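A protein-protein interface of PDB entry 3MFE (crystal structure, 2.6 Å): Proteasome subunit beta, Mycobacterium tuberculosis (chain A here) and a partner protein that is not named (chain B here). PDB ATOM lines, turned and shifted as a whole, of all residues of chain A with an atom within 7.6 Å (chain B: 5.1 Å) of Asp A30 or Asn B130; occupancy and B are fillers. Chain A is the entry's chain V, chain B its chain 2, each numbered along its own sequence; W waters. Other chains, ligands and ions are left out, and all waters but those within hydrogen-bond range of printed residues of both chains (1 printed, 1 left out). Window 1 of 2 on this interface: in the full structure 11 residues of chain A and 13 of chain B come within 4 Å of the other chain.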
ATOM      1  N   ASP A  17     -13.508  14.259   9.386  1.00  0.00           N
ATOM      2  CA  ASP A  17     -13.957  13.029   8.761  1.00  0.00           C
ATOM      3  C   ASP A  17     -13.305  12.814   7.392  1.00  0.00           C
ATOM      4  O   ASP A  17     -12.586  13.660   6.913  1.00  0.00           O
ATOM      5  CB  ASP A  17     -15.491  12.969   8.728  1.00  0.00           C
ATOM      6  CG  ASP A  17     -16.088  13.557   7.474  1.00  0.00           C
ATOM      7  OD1 ASP A  17     -16.651  12.800   6.681  1.00  0.00           O
ATOM      8  OD2 ASP A  17     -16.049  14.773   7.292  1.00  0.00           O
ATOM      9  N   ARG A  18     -13.511  11.642   6.810  1.00  0.00           N
ATOM     10  CA  ARG A  18     -12.889  11.292   5.543  1.00  0.00           C
ATOM     11  C   ARG A  18     -13.806  11.223   4.333  1.00  0.00           C
ATOM     12  O   ARG A  18     -13.352  10.937   3.246  1.00  0.00           O
ATOM     13  CB  ARG A  18     -12.164   9.964   5.691  1.00  0.00           C
ATOM     14  CG  ARG A  18     -11.365   9.860   6.947  1.00  0.00           C
ATOM     15  CD  ARG A  18     -10.181  10.779   6.927  1.00  0.00           C
ATOM     16  NE  ARG A  18      -9.211  10.350   5.945  1.00  0.00           N
ATOM     17  CZ  ARG A  18      -8.351   9.372   6.144  1.00  0.00           C
ATOM     18  NH1 ARG A  18      -8.340   8.720   7.284  1.00  0.00           N
ATOM     19  NH2 ARG A  18      -7.508   9.048   5.204  1.00  0.00           N
ATOM     20  N   ARG A  19     -15.093  11.468   4.526  1.00  0.00           N
ATOM     21  CA  ARG A  19     -16.062  11.361   3.444  1.00  0.00           C
ATOM     22  C   ARG A  19     -16.152  12.493   2.447  1.00  0.00           C
ATOM     23  O   ARG A  19     -15.996  13.652   2.768  1.00  0.00           O
ATOM     24  CB  ARG A  19     -17.456  11.082   3.974  1.00  0.00           C
ATOM     25  CG  ARG A  19     -18.501  11.139   2.891  1.00  0.00           C
ATOM     26  CD  ARG A  19     -19.771  10.489   3.306  1.00  0.00           C
ATOM     27  NE  ARG A  19     -19.540   9.128   3.734  1.00  0.00           N
ATOM     28  CZ  ARG A  19     -20.472   8.329   4.219  1.00  0.00           C
ATOM     29  NH1 ARG A  19     -21.705   8.753   4.334  1.00  0.00           N
ATOM     30  NH2 ARG A  19     -20.170   7.110   4.589  1.00  0.00           N
ATOM     31  N   SER A  20     -16.435  12.112   1.219  1.00  0.00           N
ATOM     32  CA  SER A  20     -16.681  13.034   0.141  1.00  0.00           C
ATOM     33  C   SER A  20     -17.935  12.541  -0.573  1.00  0.00           C
ATOM     34  O   SER A  20     -18.114  11.353  -0.731  1.00  0.00           O
ATOM     35  CB  SER A  20     -15.487  13.025  -0.788  1.00  0.00           C
ATOM     36  OG  SER A  20     -15.734  13.798  -1.925  1.00  0.00           O
ATOM     37  N   ILE A  26     -21.383   8.509  -2.713  1.00  0.00           N
ATOM     38  CA  ILE A  26     -20.156   8.663  -1.975  1.00  0.00           C
ATOM     39  C   ILE A  26     -19.009   8.639  -2.966  1.00  0.00           C
ATOM     40  O   ILE A  26     -18.740   7.632  -3.580  1.00  0.00           O
ATOM     41  CB  ILE A  26     -20.015   7.531  -0.938  1.00  0.00           C
ATOM     42  CG1 ILE A  26     -21.015   7.733   0.193  1.00  0.00           C
ATOM     43  CG2 ILE A  26     -18.617   7.459  -0.380  1.00  0.00           C
ATOM     44  CD1 ILE A  26     -21.272   6.528   1.016  1.00  0.00           C
ATOM     45  N   SER A  27     -18.385   9.792  -3.163  1.00  0.00           N
ATOM     46  CA  SER A  27     -17.290   9.924  -4.105  1.00  0.00           C
ATOM     47  C   SER A  27     -15.906   9.636  -3.543  1.00  0.00           C
ATOM     48  O   SER A  27     -14.982   9.375  -4.290  1.00  0.00           O
ATOM     49  CB  SER A  27     -17.327  11.291  -4.786  1.00  0.00           C
ATOM     50  OG  SER A  27     -17.137  12.349  -3.882  1.00  0.00           O
ATOM     51  N   GLY A  28     -15.759   9.704  -2.230  1.00  0.00           N
ATOM     52  CA  GLY A  28     -14.490   9.400  -1.604  1.00  0.00           C
ATOM     53  C   GLY A  28     -14.611   8.897  -0.189  1.00  0.00           C
ATOM     54  O   GLY A  28     -15.511   9.273   0.520  1.00  0.00           O
ATOM     55  N   ARG A  29     -13.687   8.040   0.209  1.00  0.00           N
ATOM     56  CA  ARG A  29     -13.661   7.503   1.554  1.00  0.00           C
ATOM     57  C   ARG A  29     -12.389   7.807   2.323  1.00  0.00           C
ATOM     58  O   ARG A  29     -12.293   7.482   3.483  1.00  0.00           O
ATOM     59  CB  ARG A  29     -13.822   5.997   1.502  1.00  0.00           C
ATOM     60  CG  ARG A  29     -15.117   5.546   0.956  1.00  0.00           C
ATOM     61  CD  ARG A  29     -15.258   4.061   1.067  1.00  0.00           C
ATOM     62  NE  ARG A  29     -16.498   3.626   0.450  1.00  0.00           N
ATOM     63  CZ  ARG A  29     -16.607   3.289  -0.821  1.00  0.00           C
ATOM     64  NH1 ARG A  29     -15.550   3.317  -1.606  1.00  0.00           N
ATOM     65  NH2 ARG A  29     -17.769   2.913  -1.303  1.00  0.00           N
ATOM     66  N   ASP A  30     -11.433   8.465   1.695  1.00  0.00           N
ATOM     67  CA  ASP A  30     -10.130   8.662   2.294  1.00  0.00           C
ATOM     68  C   ASP A  30      -9.628  10.089   2.174  1.00  0.00           C
ATOM     69  O   ASP A  30      -8.439  10.324   2.168  1.00  0.00           O
ATOM     70  CB  ASP A  30      -9.143   7.728   1.615  1.00  0.00           C
ATOM     71  CG  ASP A  30      -9.197   7.829   0.104  1.00  0.00           C
ATOM     72  OD1 ASP A  30     -10.127   8.463  -0.434  1.00  0.00           O
ATOM     73  OD2 ASP A  30      -8.302   7.285  -0.550  1.00  0.00           O
ATOM     74  N   VAL A  31     -10.544  11.034   2.063  1.00  0.00           N
ATOM     75  CA  VAL A  31     -10.204  12.439   1.947  1.00  0.00           C
ATOM     76  C   VAL A  31      -9.659  12.972   3.253  1.00  0.00           C
ATOM     77  O   VAL A  31     -10.207  12.712   4.305  1.00  0.00           O
ATOM     78  CB  VAL A  31     -11.431  13.268   1.598  1.00  0.00           C
ATOM     79  CG1 VAL A  31     -11.059  14.687   1.381  1.00  0.00           C
ATOM     80  CG2 VAL A  31     -12.107  12.712   0.401  1.00  0.00           C
ATOM     81  N   ARG A  32      -8.579  13.732   3.170  1.00  0.00           N
ATOM     82  CA  ARG A  32      -7.989  14.337   4.345  1.00  0.00           C
ATOM     83  C   ARG A  32      -8.271  15.818   4.324  1.00  0.00           C
ATOM     84  O   ARG A  32      -7.976  16.493   3.366  1.00  0.00           O
ATOM     85  CB  ARG A  32      -6.499  14.073   4.365  1.00  0.00           C
ATOM     86  CG  ARG A  32      -6.183  12.608   4.246  1.00  0.00           C
ATOM     87  CD  ARG A  32      -4.698  12.336   4.176  1.00  0.00           C
ATOM     88  NE  ARG A  32      -4.421  10.913   4.039  1.00  0.00           N
ATOM     89  CZ  ARG A  32      -4.205  10.106   5.062  1.00  0.00           C
ATOM     90  NH1 ARG A  32      -4.232  10.579   6.290  1.00  0.00           N
ATOM     91  NH2 ARG A  32      -3.961   8.829   4.860  1.00  0.00           N
ATOM     92  N   LYS A  33      -8.877  16.310   5.389  1.00  0.00           N
ATOM     93  CA  LYS A  33      -9.263  17.704   5.451  1.00  0.00           C
ATOM     94  C   LYS A  33      -8.567  18.541   6.510  1.00  0.00           C
ATOM     95  O   LYS A  33      -8.760  19.733   6.568  1.00  0.00           O
ATOM     96  CB  LYS A  33     -10.770  17.794   5.624  1.00  0.00           C
ATOM     97  CG  LYS A  33     -11.512  16.894   4.701  1.00  0.00           C
ATOM     98  CD  LYS A  33     -12.917  16.702   5.149  1.00  0.00           C
ATOM     99  CE  LYS A  33     -13.626  15.755   4.249  1.00  0.00           C
ATOM    100  NZ  LYS A  33     -14.955  15.524   4.787  1.00  0.00           N
ATOM    101  N   TYR A  35      -4.972  19.741   8.097  1.00  0.00           N
ATOM    102  CA  TYR A  35      -3.551  19.833   7.813  1.00  0.00           C
ATOM    103  C   TYR A  35      -2.780  20.752   8.740  1.00  0.00           C
ATOM    104  O   TYR A  35      -3.252  21.807   9.114  1.00  0.00           O
ATOM    105  CB  TYR A  35      -3.335  20.279   6.371  1.00  0.00           C
ATOM    106  CG  TYR A  35      -3.719  19.243   5.358  1.00  0.00           C
ATOM    107  CD1 TYR A  35      -2.860  18.205   5.044  1.00  0.00           C
ATOM    108  CD2 TYR A  35      -4.946  19.295   4.723  1.00  0.00           C
ATOM    109  CE1 TYR A  35      -3.213  17.253   4.134  1.00  0.00           C
ATOM    110  CE2 TYR A  35      -5.302  18.355   3.814  1.00  0.00           C
ATOM    111  CZ  TYR A  35      -4.433  17.337   3.516  1.00  0.00           C
ATOM    112  OH  TYR A  35      -4.789  16.397   2.592  1.00  0.00           O
ATOM    113  N   ALA A  49     -14.006  19.352  -1.180  1.00  0.00           N
ATOM    114  CA  ALA A  49     -13.098  18.451  -0.473  1.00  0.00           C
ATOM    115  C   ALA A  49     -11.751  18.248  -1.141  1.00  0.00           C
ATOM    116  O   ALA A  49     -10.735  18.146  -0.458  1.00  0.00           O
ATOM    117  CB  ALA A  49     -13.774  17.103  -0.247  1.00  0.00           C
ATOM    118  N   ALA A  50     -11.728  18.188  -2.463  1.00  0.00           N
ATOM    119  CA  ALA A  50     -10.468  18.021  -3.168  1.00  0.00           C
ATOM    120  C   ALA A  50      -9.546  19.207  -2.882  1.00  0.00           C
ATOM    121  O   ALA A  50      -8.337  19.044  -2.742  1.00  0.00           O
ATOM    122  CB  ALA A  50     -10.711  17.877  -4.657  1.00  0.00           C
ATOM    123  N   VAL A  53      -6.608  20.310   0.550  1.00  0.00           N
ATOM    124  CA  VAL A  53      -5.156  20.207   0.541  1.00  0.00           C
ATOM    125  C   VAL A  53      -4.521  21.469  -0.045  1.00  0.00           C
ATOM    126  O   VAL A  53      -3.470  21.910   0.396  1.00  0.00           O
ATOM    127  CB  VAL A  53      -4.684  18.978  -0.245  1.00  0.00           C
ATOM    128  CG1 VAL A  53      -4.840  19.216  -1.728  1.00  0.00           C
ATOM    129  CG2 VAL A  53      -3.245  18.647   0.097  1.00  0.00           C
ATOM    130  N   ILE A 190     -10.387   2.710   7.808  1.00  0.00           N
ATOM    131  CA  ILE A 190     -10.226   4.140   7.592  1.00  0.00           C
ATOM    132  C   ILE A 190     -10.913   4.902   8.711  1.00  0.00           C
ATOM    133  O   ILE A 190     -12.094   4.692   8.982  1.00  0.00           O
ATOM    134  CB  ILE A 190     -10.782   4.582   6.251  1.00  0.00           C
ATOM    135  CG1 ILE A 190     -10.157   3.723   5.135  1.00  0.00           C
ATOM    136  CG2 ILE A 190     -10.468   6.068   6.038  1.00  0.00           C
ATOM    137  CD1 ILE A 190     -10.822   3.873   3.778  1.00  0.00           C
ATOM    138  N   PHE A 191     -10.158   5.799   9.364  1.00  0.00           N
ATOM    139  CA  PHE A 191     -10.680   6.537  10.511  1.00  0.00           C
ATOM    140  C   PHE A 191     -10.478   8.021  10.328  1.00  0.00           C
ATOM    141  O   PHE A 191      -9.802   8.422   9.366  1.00  0.00           O
ATOM    142  CB  PHE A 191      -9.923   6.052  11.732  1.00  0.00           C
ATOM    143  CG  PHE A 191     -10.137   4.625  12.033  1.00  0.00           C
ATOM    144  CD1 PHE A 191     -11.201   4.252  12.824  1.00  0.00           C
ATOM    145  CD2 PHE A 191      -9.305   3.648  11.495  1.00  0.00           C
ATOM    146  CE1 PHE A 191     -11.471   2.907  13.095  1.00  0.00           C
ATOM    147  CE2 PHE A 191      -9.543   2.282  11.741  1.00  0.00           C
ATOM    148  CZ  PHE A 191     -10.638   1.904  12.547  1.00  0.00           C
ATOM    149  N   THR A 193      -9.023  11.803  10.772  1.00  0.00           N
ATOM    150  CA  THR A 193      -7.655  12.239  10.997  1.00  0.00           C
ATOM    151  C   THR A 193      -7.661  13.307  12.064  1.00  0.00           C
ATOM    152  O   THR A 193      -8.641  13.991  12.251  1.00  0.00           O
ATOM    153  CB  THR A 193      -6.935  12.767   9.737  1.00  0.00           C
ATOM    154  OG1 THR A 193      -7.575  13.936   9.244  1.00  0.00           O
ATOM    155  CG2 THR A 193      -6.886  11.738   8.672  1.00  0.00           C
ATOM    156  N   ILE B 120      -2.347   6.297  -8.079  1.00  0.00           N
ATOM    157  CA  ILE B 120      -3.520   6.656  -8.859  1.00  0.00           C
ATOM    158  C   ILE B 120      -4.025   7.961  -8.276  1.00  0.00           C
ATOM    159  O   ILE B 120      -4.353   8.038  -7.087  1.00  0.00           O
ATOM    160  CB  ILE B 120      -4.686   5.621  -8.759  1.00  0.00           C
ATOM    161  CG1 ILE B 120      -4.278   4.287  -9.367  1.00  0.00           C
ATOM    162  CG2 ILE B 120      -5.925   6.125  -9.566  1.00  0.00           C
ATOM    163  CD1 ILE B 120      -5.166   3.213  -8.937  1.00  0.00           C
ATOM    164  N   VAL B 121      -4.133   8.981  -9.119  1.00  0.00           N
ATOM    165  CA  VAL B 121      -4.628  10.292  -8.682  1.00  0.00           C
ATOM    166  C   VAL B 121      -5.824  10.751  -9.552  1.00  0.00           C
ATOM    167  O   VAL B 121      -5.755  10.724 -10.778  1.00  0.00           O
ATOM    168  CB  VAL B 121      -3.507  11.368  -8.782  1.00  0.00           C
ATOM    169  CG1 VAL B 121      -3.937  12.644  -8.110  1.00  0.00           C
ATOM    170  CG2 VAL B 121      -2.241  10.874  -8.184  1.00  0.00           C
ATOM    171  N   SER B 122      -6.901  11.188  -8.910  1.00  0.00           N
ATOM    172  CA  SER B 122      -8.098  11.647  -9.622  1.00  0.00           C
ATOM    173  C   SER B 122      -8.293  13.110  -9.348  1.00  0.00           C
ATOM    174  O   SER B 122      -7.800  13.631  -8.364  1.00  0.00           O
ATOM    175  CB  SER B 122      -9.352  10.859  -9.227  1.00  0.00           C
ATOM    176  OG  SER B 122      -9.608  10.980  -7.862  1.00  0.00           O
ATOM    177  N   GLY B 128      -9.121  19.926  -8.091  1.00  0.00           N
ATOM    178  CA  GLY B 128      -8.740  19.320  -6.834  1.00  0.00           C
ATOM    179  C   GLY B 128      -8.345  17.883  -7.053  1.00  0.00           C
ATOM    180  O   GLY B 128      -9.028  17.154  -7.789  1.00  0.00           O
ATOM    181  N   TRP B 129      -7.274  17.477  -6.375  1.00  0.00           N
ATOM    182  CA  TRP B 129      -6.755  16.129  -6.500  1.00  0.00           C
ATOM    183  C   TRP B 129      -6.942  15.250  -5.282  1.00  0.00           C
ATOM    184  O   TRP B 129      -7.052  15.755  -4.171  1.00  0.00           O
ATOM    185  CB  TRP B 129      -5.280  16.188  -6.890  1.00  0.00           C
ATOM    186  CG  TRP B 129      -4.434  16.989  -5.986  1.00  0.00           C
ATOM    187  CD1 TRP B 129      -4.294  18.348  -5.980  1.00  0.00           C
ATOM    188  CD2 TRP B 129      -3.644  16.489  -4.909  1.00  0.00           C
ATOM    189  NE1 TRP B 129      -3.470  18.722  -4.962  1.00  0.00           N
ATOM    190  CE2 TRP B 129      -3.054  17.606  -4.281  1.00  0.00           C
ATOM    191  CE3 TRP B 129      -3.393  15.202  -4.397  1.00  0.00           C
ATOM    192  CZ2 TRP B 129      -2.210  17.480  -3.141  1.00  0.00           C
ATOM    193  CZ3 TRP B 129      -2.557  15.067  -3.255  1.00  0.00           C
ATOM    194  CH2 TRP B 129      -1.977  16.207  -2.641  1.00  0.00           C
ATOM    195  N   ASN B 130      -6.913  13.937  -5.494  1.00  0.00           N
ATOM    196  CA  ASN B 130      -7.043  12.974  -4.417  1.00  0.00           C
ATOM    197  C   ASN B 130      -6.202  11.770  -4.788  1.00  0.00           C
ATOM    198  O   ASN B 130      -6.333  11.227  -5.903  1.00  0.00           O
ATOM    199  CB  ASN B 130      -8.520  12.551  -4.235  1.00  0.00           C
ATOM    200  CG  ASN B 130      -8.745  11.650  -3.005  1.00  0.00           C
ATOM    201  OD1 ASN B 130      -7.971  11.679  -2.043  1.00  0.00           O
ATOM    202  ND2 ASN B 130      -9.819  10.860  -3.037  1.00  0.00           N
ATOM    203  N   ILE B 131      -5.252  11.439  -3.904  1.00  0.00           N
ATOM    204  CA  ILE B 131      -4.445  10.239  -4.118  1.00  0.00           C
ATOM    205  C   ILE B 131      -5.293   9.119  -3.531  1.00  0.00           C
ATOM    206  O   ILE B 131      -5.597   9.123  -2.345  1.00  0.00           O
ATOM    207  CB  ILE B 131      -3.060  10.268  -3.448  1.00  0.00           C
ATOM    208  CG1 ILE B 131      -2.163  11.301  -4.128  1.00  0.00           C
ATOM    209  CG2 ILE B 131      -2.395   8.886  -3.565  1.00  0.00           C
ATOM    210  CD1 ILE B 131      -0.679  11.322  -3.563  1.00  0.00           C
ATOM    211  N   GLU B 132      -5.703   8.202  -4.408  1.00  0.00           N
ATOM    212  CA  GLU B 132      -6.553   7.059  -4.073  1.00  0.00           C
ATOM    213  C   GLU B 132      -5.857   6.017  -3.239  1.00  0.00           C
ATOM    214  O   GLU B 132      -4.808   5.487  -3.608  1.00  0.00           O
ATOM    215  CB  GLU B 132      -7.093   6.421  -5.349  1.00  0.00           C
ATOM    216  CG  GLU B 132      -7.750   7.413  -6.291  1.00  0.00           C
ATOM    217  CD  GLU B 132      -9.068   8.042  -5.776  1.00  0.00           C
ATOM    218  OE1 GLU B 132      -9.871   7.406  -5.039  1.00  0.00           O
ATOM    219  OE2 GLU B 132      -9.337   9.189  -6.171  1.00  0.00           O
ATOM    220  N   GLU B 133      -6.448   5.747  -2.091  1.00  0.00           N
ATOM    221  CA  GLU B 133      -5.918   4.776  -1.145  1.00  0.00           C
ATOM    222  C   GLU B 133      -6.669   3.422  -1.183  1.00  0.00           C
ATOM    223  O   GLU B 133      -6.291   2.474  -0.506  1.00  0.00           O
ATOM    224  CB  GLU B 133      -5.967   5.404   0.260  1.00  0.00           C
ATOM    225  CG  GLU B 133      -5.123   6.705   0.409  1.00  0.00           C
ATOM    226  CD  GLU B 133      -5.240   7.406   1.770  1.00  0.00           C
ATOM    227  OE1 GLU B 133      -5.108   8.654   1.779  1.00  0.00           O
ATOM    228  OE2 GLU B 133      -5.450   6.736   2.817  1.00  0.00           O
ATOM    229  N   GLU B 134      -7.680   3.323  -2.042  1.00  0.00           N
ATOM    230  CA  GLU B 134      -8.513   2.134  -2.148  1.00  0.00           C
ATOM    231  C   GLU B 134      -8.031   1.092  -3.163  1.00  0.00           C
ATOM    232  O   GLU B 134      -8.550  -0.010  -3.179  1.00  0.00           O
ATOM    233  CB  GLU B 134      -9.971   2.552  -2.412  1.00  0.00           C
ATOM    234  CG  GLU B 134     -11.056   1.573  -1.941  1.00  0.00           C
ATOM    235  CD  GLU B 134     -12.487   2.124  -2.107  1.00  0.00           C
ATOM    236  OE1 GLU B 134     -12.997   2.230  -3.260  1.00  0.00           O
ATOM    237  OE2 GLU B 134     -13.095   2.446  -1.060  1.00  0.00           O
HETATM  238  O   HOH W   1     -12.984  11.971  -3.733  1.00  0.00           O
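The side-chain carboxylate of Asp A30 lies within hydrogen-bond range of the backbone NH of Glu B133.
OE2 of Glu B133 is in salt-bridge range of NH2 of Arg A18 (3.9 Å).
The side-chain carboxylate of Glu B133 lies within salt-bridge range of the guanidinium group of Arg A32 (3.3 Å).
OE2 of Glu B134 is in salt-bridge range of NH1 of Arg A29, at 2.7 Å.
N of Asn B130 lies within hydrogen-bond range of O of Ser B122 (3.0 Å).
The guanidinium group of Arg A18 is in hydrogen-bond range of the backbone carbonyl oxygen of Asp A30 (3.4 Å).
O of Val A31 sits at hydrogen-bond distance from NE of Arg A18 (3.0 Å).
The backbone carbonyl oxygen of Arg A32 is in hydrogen-bond range of the side-chain hydroxyl of Tyr A35.
The side-chain hydroxyl (OG) of Ser B122 sits at hydrogen-bond distance from the side-chain carboxylate (OE2) of Glu B132 (2.5 Å).
The backbone carbonyl oxygen (O) of Phe A191 is in hydrogen-bond range of the guanidinium group (NH1) of Arg A18, at 2.6 Å.
Among the printed residues, merely in contact across the chains: Asp A30 with Asn B130 (3.6 Å), Asp A30 with Ile B131 (3.7 Å), Asp A30 with Glu B132 (3.8 Å), Ala A50 with Gly B128 (3.3 Å), Ala A50 with Trp B129 (3.8 Å) and Val A53 with Trp B129 (3.5 Å).
Asp A30 touches just these residues of chain B: Asn B130, Ile B131, Glu B132 and Glu B133.
Of chain A, only Asp A30 (3.6 Å) comes within 4 Å of Asn B130.
Printed residues of chain B within 4 Å of Ala A50: Gly B128 (3.3 Å) and Trp B129 (3.8 Å).
Of the printed residues of chain B, Val A53 touches Trp B129.
Of the printed residues of chain B, Arg A32 touches Glu B133.
Printed residues of chain A within 4 Å of Ile B131: Asp A30.
Printed residues of chain B within 4 Å of Arg A29: Glu B134 (2.7 Å).
The nearest residue of chain A that does not touch Asn B130 is Val A31 (4.5 Å).
Of the 10 printed residues of chain B, 7 touch a printed residue of chain A.
Among the printed residues, Asp or Glu carboxylates within 4 Å of a Lys or Arg side-chain nitrogen of the other chain: Arg A18 with Glu B133, Arg A29 with Glu B134 and Arg A32 with Glu B133.
Water W1 lies within hydrogen-bond range of O of Ser A27 (3.3 Å) and ND2 of Asn B130 (3.4 Å).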
